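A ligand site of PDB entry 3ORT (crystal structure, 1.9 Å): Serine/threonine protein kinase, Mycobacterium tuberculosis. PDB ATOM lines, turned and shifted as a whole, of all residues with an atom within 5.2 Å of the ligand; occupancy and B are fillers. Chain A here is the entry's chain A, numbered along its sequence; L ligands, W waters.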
ATOM      1  N   LEU A  20      -3.831 -20.087 -11.830  1.00  0.00           N
ATOM      2  CA  LEU A  20      -2.822 -20.507 -10.851  1.00  0.00           C
ATOM      3  C   LEU A  20      -2.966 -19.791  -9.529  1.00  0.00           C
ATOM      4  O   LEU A  20      -2.734 -20.368  -8.467  1.00  0.00           O
ATOM      5  CB  LEU A  20      -1.419 -20.239 -11.420  1.00  0.00           C
ATOM      6  CG  LEU A  20      -0.989 -21.068 -12.630  1.00  0.00           C
ATOM      7  CD1 LEU A  20       0.317 -20.510 -13.215  1.00  0.00           C
ATOM      8  CD2 LEU A  20      -0.860 -22.558 -12.275  1.00  0.00           C
ATOM      9  N   GLY A  21      -3.316 -18.514  -9.592  1.00  0.00           N
ATOM     10  CA  GLY A  21      -3.380 -17.709  -8.397  1.00  0.00           C
ATOM     11  C   GLY A  21      -4.034 -16.369  -8.647  1.00  0.00           C
ATOM     12  O   GLY A  21      -4.342 -16.022  -9.789  1.00  0.00           O
ATOM     13  N   PHE A  22      -4.313 -15.661  -7.569  1.00  0.00           N
ATOM     14  CA  PHE A  22      -4.750 -14.281  -7.623  1.00  0.00           C
ATOM     15  C   PHE A  22      -4.306 -13.507  -6.375  1.00  0.00           C
ATOM     16  O   PHE A  22      -3.939 -14.084  -5.336  1.00  0.00           O
ATOM     17  CB  PHE A  22      -6.258 -14.186  -7.832  1.00  0.00           C
ATOM     18  CG  PHE A  22      -7.063 -14.468  -6.588  1.00  0.00           C
ATOM     19  CD1 PHE A  22      -7.572 -13.429  -5.806  1.00  0.00           C
ATOM     20  CD2 PHE A  22      -7.310 -15.785  -6.190  1.00  0.00           C
ATOM     21  CE1 PHE A  22      -8.320 -13.682  -4.658  1.00  0.00           C
ATOM     22  CE2 PHE A  22      -8.053 -16.055  -5.029  1.00  0.00           C
ATOM     23  CZ  PHE A  22      -8.565 -14.991  -4.266  1.00  0.00           C
ATOM     24  N   GLY A  23      -4.297 -12.196  -6.497  1.00  0.00           N
ATOM     25  CA  GLY A  23      -3.808 -11.353  -5.449  1.00  0.00           C
ATOM     26  C   GLY A  23      -4.716 -10.172  -5.310  1.00  0.00           C
ATOM     27  O   GLY A  23      -5.856 -10.195  -5.765  1.00  0.00           O
ATOM     28  N   GLY A  24      -4.183  -9.120  -4.702  1.00  0.00           N
ATOM     29  CA  GLY A  24      -4.908  -7.881  -4.492  1.00  0.00           C
ATOM     30  C   GLY A  24      -5.447  -7.293  -5.777  1.00  0.00           C
ATOM     31  O   GLY A  24      -6.584  -6.808  -5.799  1.00  0.00           O
ATOM     32  N   MET A  25      -4.640  -7.327  -6.850  1.00  0.00           N
ATOM     33  CA  MET A  25      -5.055  -6.733  -8.137  1.00  0.00           C
ATOM     34  C   MET A  25      -5.027  -7.655  -9.346  1.00  0.00           C
ATOM     35  O   MET A  25      -5.546  -7.268 -10.383  1.00  0.00           O
ATOM     36  CB  MET A  25      -4.200  -5.508  -8.461  1.00  0.00           C
ATOM     37  CG  MET A  25      -2.800  -5.833  -8.978  1.00  0.00           C
ATOM     38  SD  MET A  25      -1.747  -4.397  -9.157  1.00  0.00           S
ATOM     39  CE  MET A  25      -3.009  -3.221  -9.553  1.00  0.00           C
ATOM     40  N   SER A  26      -4.412  -8.834  -9.253  1.00  0.00           N
ATOM     41  CA  SER A  26      -4.310  -9.659 -10.445  1.00  0.00           C
ATOM     42  C   SER A  26      -4.590 -11.127 -10.297  1.00  0.00           C
ATOM     43  O   SER A  26      -4.681 -11.652  -9.201  1.00  0.00           O
ATOM     44  CB  SER A  26      -2.970  -9.454 -11.155  1.00  0.00           C
ATOM     45  OG  SER A  26      -1.932  -9.214 -10.265  1.00  0.00           O
ATOM     46  N   VAL A  28      -3.317 -14.827 -12.040  1.00  0.00           N
ATOM     47  CA  VAL A  28      -2.234 -15.447 -12.752  1.00  0.00           C
ATOM     48  C   VAL A  28      -2.734 -16.772 -13.308  1.00  0.00           C
ATOM     49  O   VAL A  28      -3.365 -17.560 -12.608  1.00  0.00           O
ATOM     50  CB  VAL A  28      -0.976 -15.592 -11.886  1.00  0.00           C
ATOM     51  CG1 VAL A  28       0.222 -16.151 -12.717  1.00  0.00           C
ATOM     52  CG2 VAL A  28      -0.617 -14.242 -11.239  1.00  0.00           C
ATOM     53  N   ALA A  41       3.635 -18.055 -17.268  1.00  0.00           N
ATOM     54  CA  ALA A  41       2.611 -17.514 -16.385  1.00  0.00           C
ATOM     55  C   ALA A  41       2.251 -16.158 -16.929  1.00  0.00           C
ATOM     56  O   ALA A  41       3.117 -15.357 -17.276  1.00  0.00           O
ATOM     57  CB  ALA A  41       3.118 -17.380 -14.938  1.00  0.00           C
ATOM     58  N   LYS A  43       0.169 -12.833 -15.874  1.00  0.00           N
ATOM     59  CA  LYS A  43      -0.506 -12.076 -14.825  1.00  0.00           C
ATOM     60  C   LYS A  43      -1.322 -11.014 -15.505  1.00  0.00           C
ATOM     61  O   LYS A  43      -0.823 -10.267 -16.337  1.00  0.00           O
ATOM     62  CB  LYS A  43       0.493 -11.442 -13.878  1.00  0.00           C
ATOM     63  CG  LYS A  43      -0.132 -10.602 -12.802  1.00  0.00           C
ATOM     64  CD  LYS A  43       0.910  -9.929 -11.908  1.00  0.00           C
ATOM     65  CE  LYS A  43       1.692 -10.919 -11.107  1.00  0.00           C
ATOM     66  NZ  LYS A  43       2.476 -10.232 -10.003  1.00  0.00           N
ATOM     67  N   ARG A  58      -2.984   1.144 -11.208  1.00  0.00           N
ATOM     68  CA  ARG A  58      -2.064   0.462 -10.322  1.00  0.00           C
ATOM     69  C   ARG A  58      -1.407  -0.664 -11.088  1.00  0.00           C
ATOM     70  O   ARG A  58      -0.201  -0.849 -11.014  1.00  0.00           O
ATOM     71  CB  ARG A  58      -2.766  -0.069  -9.055  1.00  0.00           C
ATOM     72  CG  ARG A  58      -3.109   1.005  -8.000  1.00  0.00           C
ATOM     73  CD  ARG A  58      -3.410   0.415  -6.597  1.00  0.00           C
ATOM     74  NE  ARG A  58      -2.336  -0.477  -6.152  1.00  0.00           N
ATOM     75  CZ  ARG A  58      -2.418  -1.394  -5.191  1.00  0.00           C
ATOM     76  NH1 ARG A  58      -3.548  -1.573  -4.498  1.00  0.00           N
ATOM     77  NH2 ARG A  58      -1.366  -2.156  -4.903  1.00  0.00           N
ATOM     78  N   ALA A  63       2.442  -3.736 -11.118  1.00  0.00           N
ATOM     79  CA  ALA A  63       2.617  -5.142 -11.546  1.00  0.00           C
ATOM     80  C   ALA A  63       3.403  -5.244 -12.854  1.00  0.00           C
ATOM     81  O   ALA A  63       4.355  -6.057 -12.978  1.00  0.00           O
ATOM     82  CB  ALA A  63       1.240  -5.830 -11.711  1.00  0.00           C
ATOM     83  N   VAL A  75      12.266 -14.962 -10.775  1.00  0.00           N
ATOM     84  CA  VAL A  75      11.256 -15.251 -11.790  1.00  0.00           C
ATOM     85  C   VAL A  75      11.480 -14.281 -12.926  1.00  0.00           C
ATOM     86  O   VAL A  75      11.336 -13.052 -12.729  1.00  0.00           O
ATOM     87  CB  VAL A  75       9.821 -15.077 -11.249  1.00  0.00           C
ATOM     88  CG1 VAL A  75       8.761 -15.177 -12.367  1.00  0.00           C
ATOM     89  CG2 VAL A  75       9.574 -16.133 -10.187  1.00  0.00           C
ATOM     90  N   MET A  95       5.496 -13.915 -17.632  1.00  0.00           N
ATOM     91  CA  MET A  95       6.706 -14.280 -16.891  1.00  0.00           C
ATOM     92  C   MET A  95       6.928 -15.774 -16.805  1.00  0.00           C
ATOM     93  O   MET A  95       6.066 -16.596 -17.189  1.00  0.00           O
ATOM     94  CB  MET A  95       6.631 -13.691 -15.462  1.00  0.00           C
ATOM     95  CG  MET A  95       5.552 -14.303 -14.635  1.00  0.00           C
ATOM     96  SD  MET A  95       5.075 -13.214 -13.294  1.00  0.00           S
ATOM     97  CE  MET A  95       3.329 -13.277 -13.589  1.00  0.00           C
ATOM     98  N   GLU A  96       8.085 -16.108 -16.261  1.00  0.00           N
ATOM     99  CA  GLU A  96       8.469 -17.496 -16.028  1.00  0.00           C
ATOM    100  C   GLU A  96       7.406 -18.174 -15.166  1.00  0.00           C
ATOM    101  O   GLU A  96       6.960 -17.608 -14.146  1.00  0.00           O
ATOM    102  CB  GLU A  96       9.824 -17.552 -15.352  1.00  0.00           C
ATOM    103  CG  GLU A  96      10.238 -18.899 -14.813  1.00  0.00           C
ATOM    104  CD  GLU A  96      11.601 -18.870 -14.174  1.00  0.00           C
ATOM    105  OE1 GLU A  96      12.301 -17.826 -14.279  1.00  0.00           O
ATOM    106  OE2 GLU A  96      11.962 -19.897 -13.562  1.00  0.00           O
ATOM    107  N   TYR A  97       7.001 -19.368 -15.581  1.00  0.00           N
ATOM    108  CA  TYR A  97       6.050 -20.220 -14.850  1.00  0.00           C
ATOM    109  C   TYR A  97       6.764 -20.993 -13.725  1.00  0.00           C
ATOM    110  O   TYR A  97       7.787 -21.631 -13.965  1.00  0.00           O
ATOM    111  CB  TYR A  97       5.388 -21.205 -15.820  1.00  0.00           C
ATOM    112  CG  TYR A  97       4.638 -22.321 -15.141  1.00  0.00           C
ATOM    113  CD1 TYR A  97       3.616 -22.061 -14.212  1.00  0.00           C
ATOM    114  CD2 TYR A  97       4.918 -23.662 -15.429  1.00  0.00           C
ATOM    115  CE1 TYR A  97       2.913 -23.105 -13.573  1.00  0.00           C
ATOM    116  CE2 TYR A  97       4.228 -24.690 -14.801  1.00  0.00           C
ATOM    117  CZ  TYR A  97       3.223 -24.403 -13.880  1.00  0.00           C
ATOM    118  OH  TYR A  97       2.533 -25.438 -13.260  1.00  0.00           O
ATOM    119  N   VAL A  98       6.201 -20.919 -12.518  1.00  0.00           N
ATOM    120  CA  VAL A  98       6.652 -21.667 -11.377  1.00  0.00           C
ATOM    121  C   VAL A  98       5.524 -22.608 -10.980  1.00  0.00           C
ATOM    122  O   VAL A  98       4.433 -22.180 -10.599  1.00  0.00           O
ATOM    123  CB  VAL A  98       7.046 -20.768 -10.147  1.00  0.00           C
ATOM    124  CG1 VAL A  98       7.549 -21.640  -9.002  1.00  0.00           C
ATOM    125  CG2 VAL A  98       8.110 -19.763 -10.530  1.00  0.00           C
ATOM    126  N   THR A 102       3.691 -20.199  -2.958  1.00  0.00           N
ATOM    127  CA  THR A 102       4.338 -19.054  -2.255  1.00  0.00           C
ATOM    128  C   THR A 102       4.618 -19.410  -0.809  1.00  0.00           C
ATOM    129  O   THR A 102       3.930 -20.270  -0.243  1.00  0.00           O
ATOM    130  CB  THR A 102       3.482 -17.766  -2.245  1.00  0.00           C
ATOM    131  OG1 THR A 102       2.297 -17.967  -1.462  1.00  0.00           O
ATOM    132  CG2 THR A 102       3.088 -17.329  -3.653  1.00  0.00           C
ATOM    133  N   ASP A 105       1.434 -18.975   1.287  1.00  0.00           N
ATOM    134  CA  ASP A 105       0.612 -20.173   1.280  1.00  0.00           C
ATOM    135  C   ASP A 105       1.172 -21.315   2.128  1.00  0.00           C
ATOM    136  O   ASP A 105       0.416 -22.003   2.802  1.00  0.00           O
ATOM    137  CB  ASP A 105       0.390 -20.631  -0.137  1.00  0.00           C
ATOM    138  CG  ASP A 105      -0.588 -19.735  -0.871  1.00  0.00           C
ATOM    139  OD1 ASP A 105      -1.315 -18.953  -0.200  1.00  0.00           O
ATOM    140  OD2 ASP A 105      -0.633 -19.811  -2.107  1.00  0.00           O
ATOM    141  N   ASP A 141       9.857  -4.851  -2.029  1.00  0.00           N
ATOM    142  CA  ASP A 141       8.630  -5.498  -1.539  1.00  0.00           C
ATOM    143  C   ASP A 141       8.842  -6.955  -1.233  1.00  0.00           C
ATOM    144  O   ASP A 141       8.057  -7.820  -1.634  1.00  0.00           O
ATOM    145  CB  ASP A 141       7.510  -5.363  -2.546  1.00  0.00           C
ATOM    146  CG  ASP A 141       6.101  -5.482  -1.913  1.00  0.00           C
ATOM    147  OD1 ASP A 141       5.958  -5.247  -0.696  1.00  0.00           O
ATOM    148  OD2 ASP A 141       5.137  -5.778  -2.648  1.00  0.00           O
ATOM    149  N   LYS A 143       8.419 -10.073   0.716  1.00  0.00           N
ATOM    150  CA  LYS A 143       7.321 -10.539   1.546  1.00  0.00           C
ATOM    151  C   LYS A 143       7.095 -11.995   1.177  1.00  0.00           C
ATOM    152  O   LYS A 143       7.563 -12.437   0.128  1.00  0.00           O
ATOM    153  CB  LYS A 143       6.038  -9.681   1.347  1.00  0.00           C
ATOM    154  CG  LYS A 143       5.534  -9.640  -0.068  1.00  0.00           C
ATOM    155  CD  LYS A 143       4.485  -8.589  -0.270  1.00  0.00           C
ATOM    156  CE  LYS A 143       3.726  -8.845  -1.555  1.00  0.00           C
ATOM    157  NZ  LYS A 143       2.703  -7.791  -1.797  1.00  0.00           N
ATOM    158  N   ALA A 145       4.597 -13.505   0.078  1.00  0.00           N
ATOM    159  CA  ALA A 145       3.871 -13.709  -1.158  1.00  0.00           C
ATOM    160  C   ALA A 145       4.748 -13.630  -2.414  1.00  0.00           C
ATOM    161  O   ALA A 145       4.305 -14.069  -3.499  1.00  0.00           O
ATOM    162  CB  ALA A 145       2.712 -12.743  -1.237  1.00  0.00           C
ATOM    163  N   ASN A 146       5.960 -13.058  -2.289  1.00  0.00           N
ATOM    164  CA  ASN A 146       6.848 -12.824  -3.434  1.00  0.00           C
ATOM    165  C   ASN A 146       7.978 -13.828  -3.502  1.00  0.00           C
ATOM    166  O   ASN A 146       8.932 -13.646  -4.248  1.00  0.00           O
ATOM    167  CB  ASN A 146       7.422 -11.412  -3.389  1.00  0.00           C
ATOM    168  CG  ASN A 146       6.516 -10.380  -4.036  1.00  0.00           C
ATOM    169  OD1 ASN A 146       5.720 -10.703  -4.924  1.00  0.00           O
ATOM    170  ND2 ASN A 146       6.630  -9.131  -3.590  1.00  0.00           N
ATOM    171  N   MET A 148       8.361 -18.103  -3.997  1.00  0.00           N
ATOM    172  CA  MET A 148       7.766 -19.437  -4.200  1.00  0.00           C
ATOM    173  C   MET A 148       8.783 -20.542  -4.045  1.00  0.00           C
ATOM    174  O   MET A 148       9.966 -20.366  -4.262  1.00  0.00           O
ATOM    175  CB  MET A 148       7.124 -19.554  -5.599  1.00  0.00           C
ATOM    176  CG  MET A 148       6.059 -18.472  -5.886  1.00  0.00           C
ATOM    177  SD  MET A 148       5.194 -18.594  -7.470  1.00  0.00           S
ATOM    178  CE  MET A 148       4.402 -20.206  -7.308  1.00  0.00           C
ATOM    179  N   MET A 158      10.232 -13.019  -6.873  1.00  0.00           N
ATOM    180  CA  MET A 158       9.553 -12.308  -7.951  1.00  0.00           C
ATOM    181  C   MET A 158       9.150 -10.906  -7.586  1.00  0.00           C
ATOM    182  O   MET A 158       9.176 -10.546  -6.434  1.00  0.00           O
ATOM    183  CB  MET A 158       8.329 -13.105  -8.420  1.00  0.00           C
ATOM    184  CG  MET A 158       7.294 -13.364  -7.357  1.00  0.00           C
ATOM    185  SD  MET A 158       6.195 -14.665  -7.886  1.00  0.00           S
ATOM    186  CE  MET A 158       4.718 -14.370  -6.851  1.00  0.00           C
ATOM    187  N   ASP A 159       8.812 -10.137  -8.629  1.00  0.00           N
ATOM    188  CA  ASP A 159       8.164  -8.849  -8.567  1.00  0.00           C
ATOM    189  C   ASP A 159       9.075  -7.782  -7.953  1.00  0.00           C
ATOM    190  O   ASP A 159       8.731  -7.174  -6.964  1.00  0.00           O
ATOM    191  CB  ASP A 159       6.788  -8.980  -7.888  1.00  0.00           C
ATOM    192  CG  ASP A 159       5.805  -9.828  -8.726  1.00  0.00           C
ATOM    193  OD1 ASP A 159       5.920  -9.807  -9.983  1.00  0.00           O
ATOM    194  OD2 ASP A 159       4.898 -10.516  -8.153  1.00  0.00           O
HETATM  195  P1  LIG L   1      -0.277  -8.085  -4.717  1.00  0.00           P
HETATM  196  S1  LIG L   1      -0.996  -6.615  -5.188  1.00  0.00           S
HETATM  197  O1  LIG L   1      -1.310  -8.820  -3.837  1.00  0.00           O
HETATM  198  O2  LIG L   1       1.140  -7.756  -4.150  1.00  0.00           O
HETATM  199  P2  LIG L   1      -0.850  -9.407  -7.252  1.00  0.00           P
HETATM  200  O3  LIG L   1      -2.284  -9.046  -7.161  1.00  0.00           O
HETATM  201  O4  LIG L   1      -0.147  -8.827  -8.469  1.00  0.00           O
HETATM  202  O5  LIG L   1       0.037  -9.091  -5.948  1.00  0.00           O
HETATM  203  P3  LIG L   1       0.651 -11.822  -6.934  1.00  0.00           P
HETATM  204  O6  LIG L   1       1.831 -11.166  -7.530  1.00  0.00           O
HETATM  205  O7  LIG L   1       0.732 -12.097  -5.425  1.00  0.00           O
HETATM  206  O8  LIG L   1      -0.682 -11.001  -7.267  1.00  0.00           O
HETATM  207  O9  LIG L   1       0.275 -13.216  -7.662  1.00  0.00           O
HETATM  208  C1  LIG L   1      -0.895 -13.898  -7.269  1.00  0.00           C
HETATM  209  C2  LIG L   1      -0.645 -15.387  -7.150  1.00  0.00           C
HETATM  210  O10 LIG L   1      -0.352 -15.904  -8.444  1.00  0.00           O
HETATM  211  C3  LIG L   1       0.539 -15.807  -6.268  1.00  0.00           C
HETATM  212  O11 LIG L   1       0.216 -16.060  -4.929  1.00  0.00           O
HETATM  213  C4  LIG L   1       0.911 -17.121  -6.936  1.00  0.00           C
HETATM  214  O12 LIG L   1       0.053 -18.157  -6.528  1.00  0.00           O
HETATM  215  C5  LIG L   1       0.605 -16.947  -8.397  1.00  0.00           C
HETATM  216  N1  LIG L   1       1.777 -16.563  -9.178  1.00  0.00           N
HETATM  217  C6  LIG L   1       2.332 -15.305  -9.331  1.00  0.00           C
HETATM  218  N2  LIG L   1       3.382 -15.371 -10.178  1.00  0.00           N
HETATM  219  C7  LIG L   1       3.545 -16.648 -10.589  1.00  0.00           C
HETATM  220  C8  LIG L   1       4.407 -17.307 -11.461  1.00  0.00           C
HETATM  221  N3  LIG L   1       5.604 -16.875 -11.805  1.00  0.00           N
HETATM  222  N4  LIG L   1       4.254 -18.655 -11.624  1.00  0.00           N
HETATM  223  C9  LIG L   1       3.251 -19.331 -10.998  1.00  0.00           C
HETATM  224  N5  LIG L   1       2.391 -18.682 -10.156  1.00  0.00           N
HETATM  225  C10 LIG L   1       2.521 -17.383  -9.945  1.00  0.00           C
HETATM  226  O   HOH W   1       4.384 -12.554 -10.060  1.00  0.00           O
HETATM  227  O   HOH W   2       2.373  -7.283  -8.588  1.00  0.00           O
HETATM  228  O   HOH W   3       2.420 -10.433  -4.088  1.00  0.00           O
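The backbone NH (N) of Ser 26 is in hydrogen-bond range of an oxygen (O3) of the ligand (3.0 Å). An oxygen (O4) of the ligand is in hydrogen-bond range of the side-chain hydroxyl (OG) of Ser 26. NZ of Lys 43 lies within salt-bridge range of O6 of the ligand, 2.7 Å away. The backbone carbonyl oxygen (O) of Glu 96 sits at hydrogen-bond distance from a nitrogen (N3) of the ligand. An oxygen (O2) of the ligand lies within hydrogen-bond range of the side-chain amino group (NZ) of Lys 143 (2.8 Å). N of Met 25 sits at hydrogen-bond distance from O3 of the ligand (2.9 Å). N of Gly 24 is in hydrogen-bond range of O1 of the ligand (3.0 Å). A nitrogen (N4) of the ligand is in hydrogen-bond range of the backbone NH (N) of Val 98 (3.1 Å).
The side-chain amino group (NZ) of Lys 43 is in salt-bridge range of the side-chain carboxylate (OD2) of Asp 159 (3.1 Å). NZ of Lys 143 is in salt-bridge range of OD2 of Asp 141 (3.3 Å). The side-chain carboxylate (OD2) of Asp 159 lies close to the side-chain amide oxygen (OD1) of Asn 146 (3.3 Å). The backbone NH (N) of Val 28 is in hydrogen-bond range of the backbone carbonyl oxygen (O) of Gly 21 (2.7 Å). O of Val 28 is in hydrogen-bond range of N of Leu 20, 2.7 Å away. N of Asp 105 is in hydrogen-bond range of OG1 of Thr 102 (3.1 Å). The backbone NH (N) of Met 158 lies within hydrogen-bond range of the backbone carbonyl oxygen (O) of Asn 146 (3.0 Å). The backbone NH (N) of Met 95 lies within hydrogen-bond range of the backbone carbonyl oxygen (O) of Ala 41, 2.8 Å away.
The side-chain sulfur of Met 158 sits close to a nitrogen (N2) of the ligand, at 3.7 Å. An oxygen (O6) of the ligand lies close to the side-chain carboxylate of Asp 159. CD1 of Leu 20 touches C9 of the ligand (3.9 Å). Gly 21 touches the ligand (CA to O10, 3.5 Å). Phe 22 touches the ligand (C to C1, 3.5 Å). Gly 23 touches the ligand. Val 28 touches the ligand (CG2 to O10, 3.3 Å). CB of Ala 41 touches C8 of the ligand (3.7 Å). CG1 of Val 75 touches N3 of the ligand, at 3.6 Å. Met 95 touches the ligand. Thr 102 touches the ligand. Met 148 touches the ligand (CE to N5, 3.8 Å). Hydrophobic or aromatic side chains within 4 Å of the ligand: Leu 20, Met 25, Val 28, Ala 41, Val 75, Met 95, Val 98, Met 148 and Met 158. Of the 26 residues printed, 19 come within 4 Å of the ligand.
Water W3 lies within hydrogen-bond range of O7 of the ligand (2.7 Å) and OD1 of Asn 146 (3.4 Å). Water W2 bridges O4 of the ligand and NZ of Lys 43.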
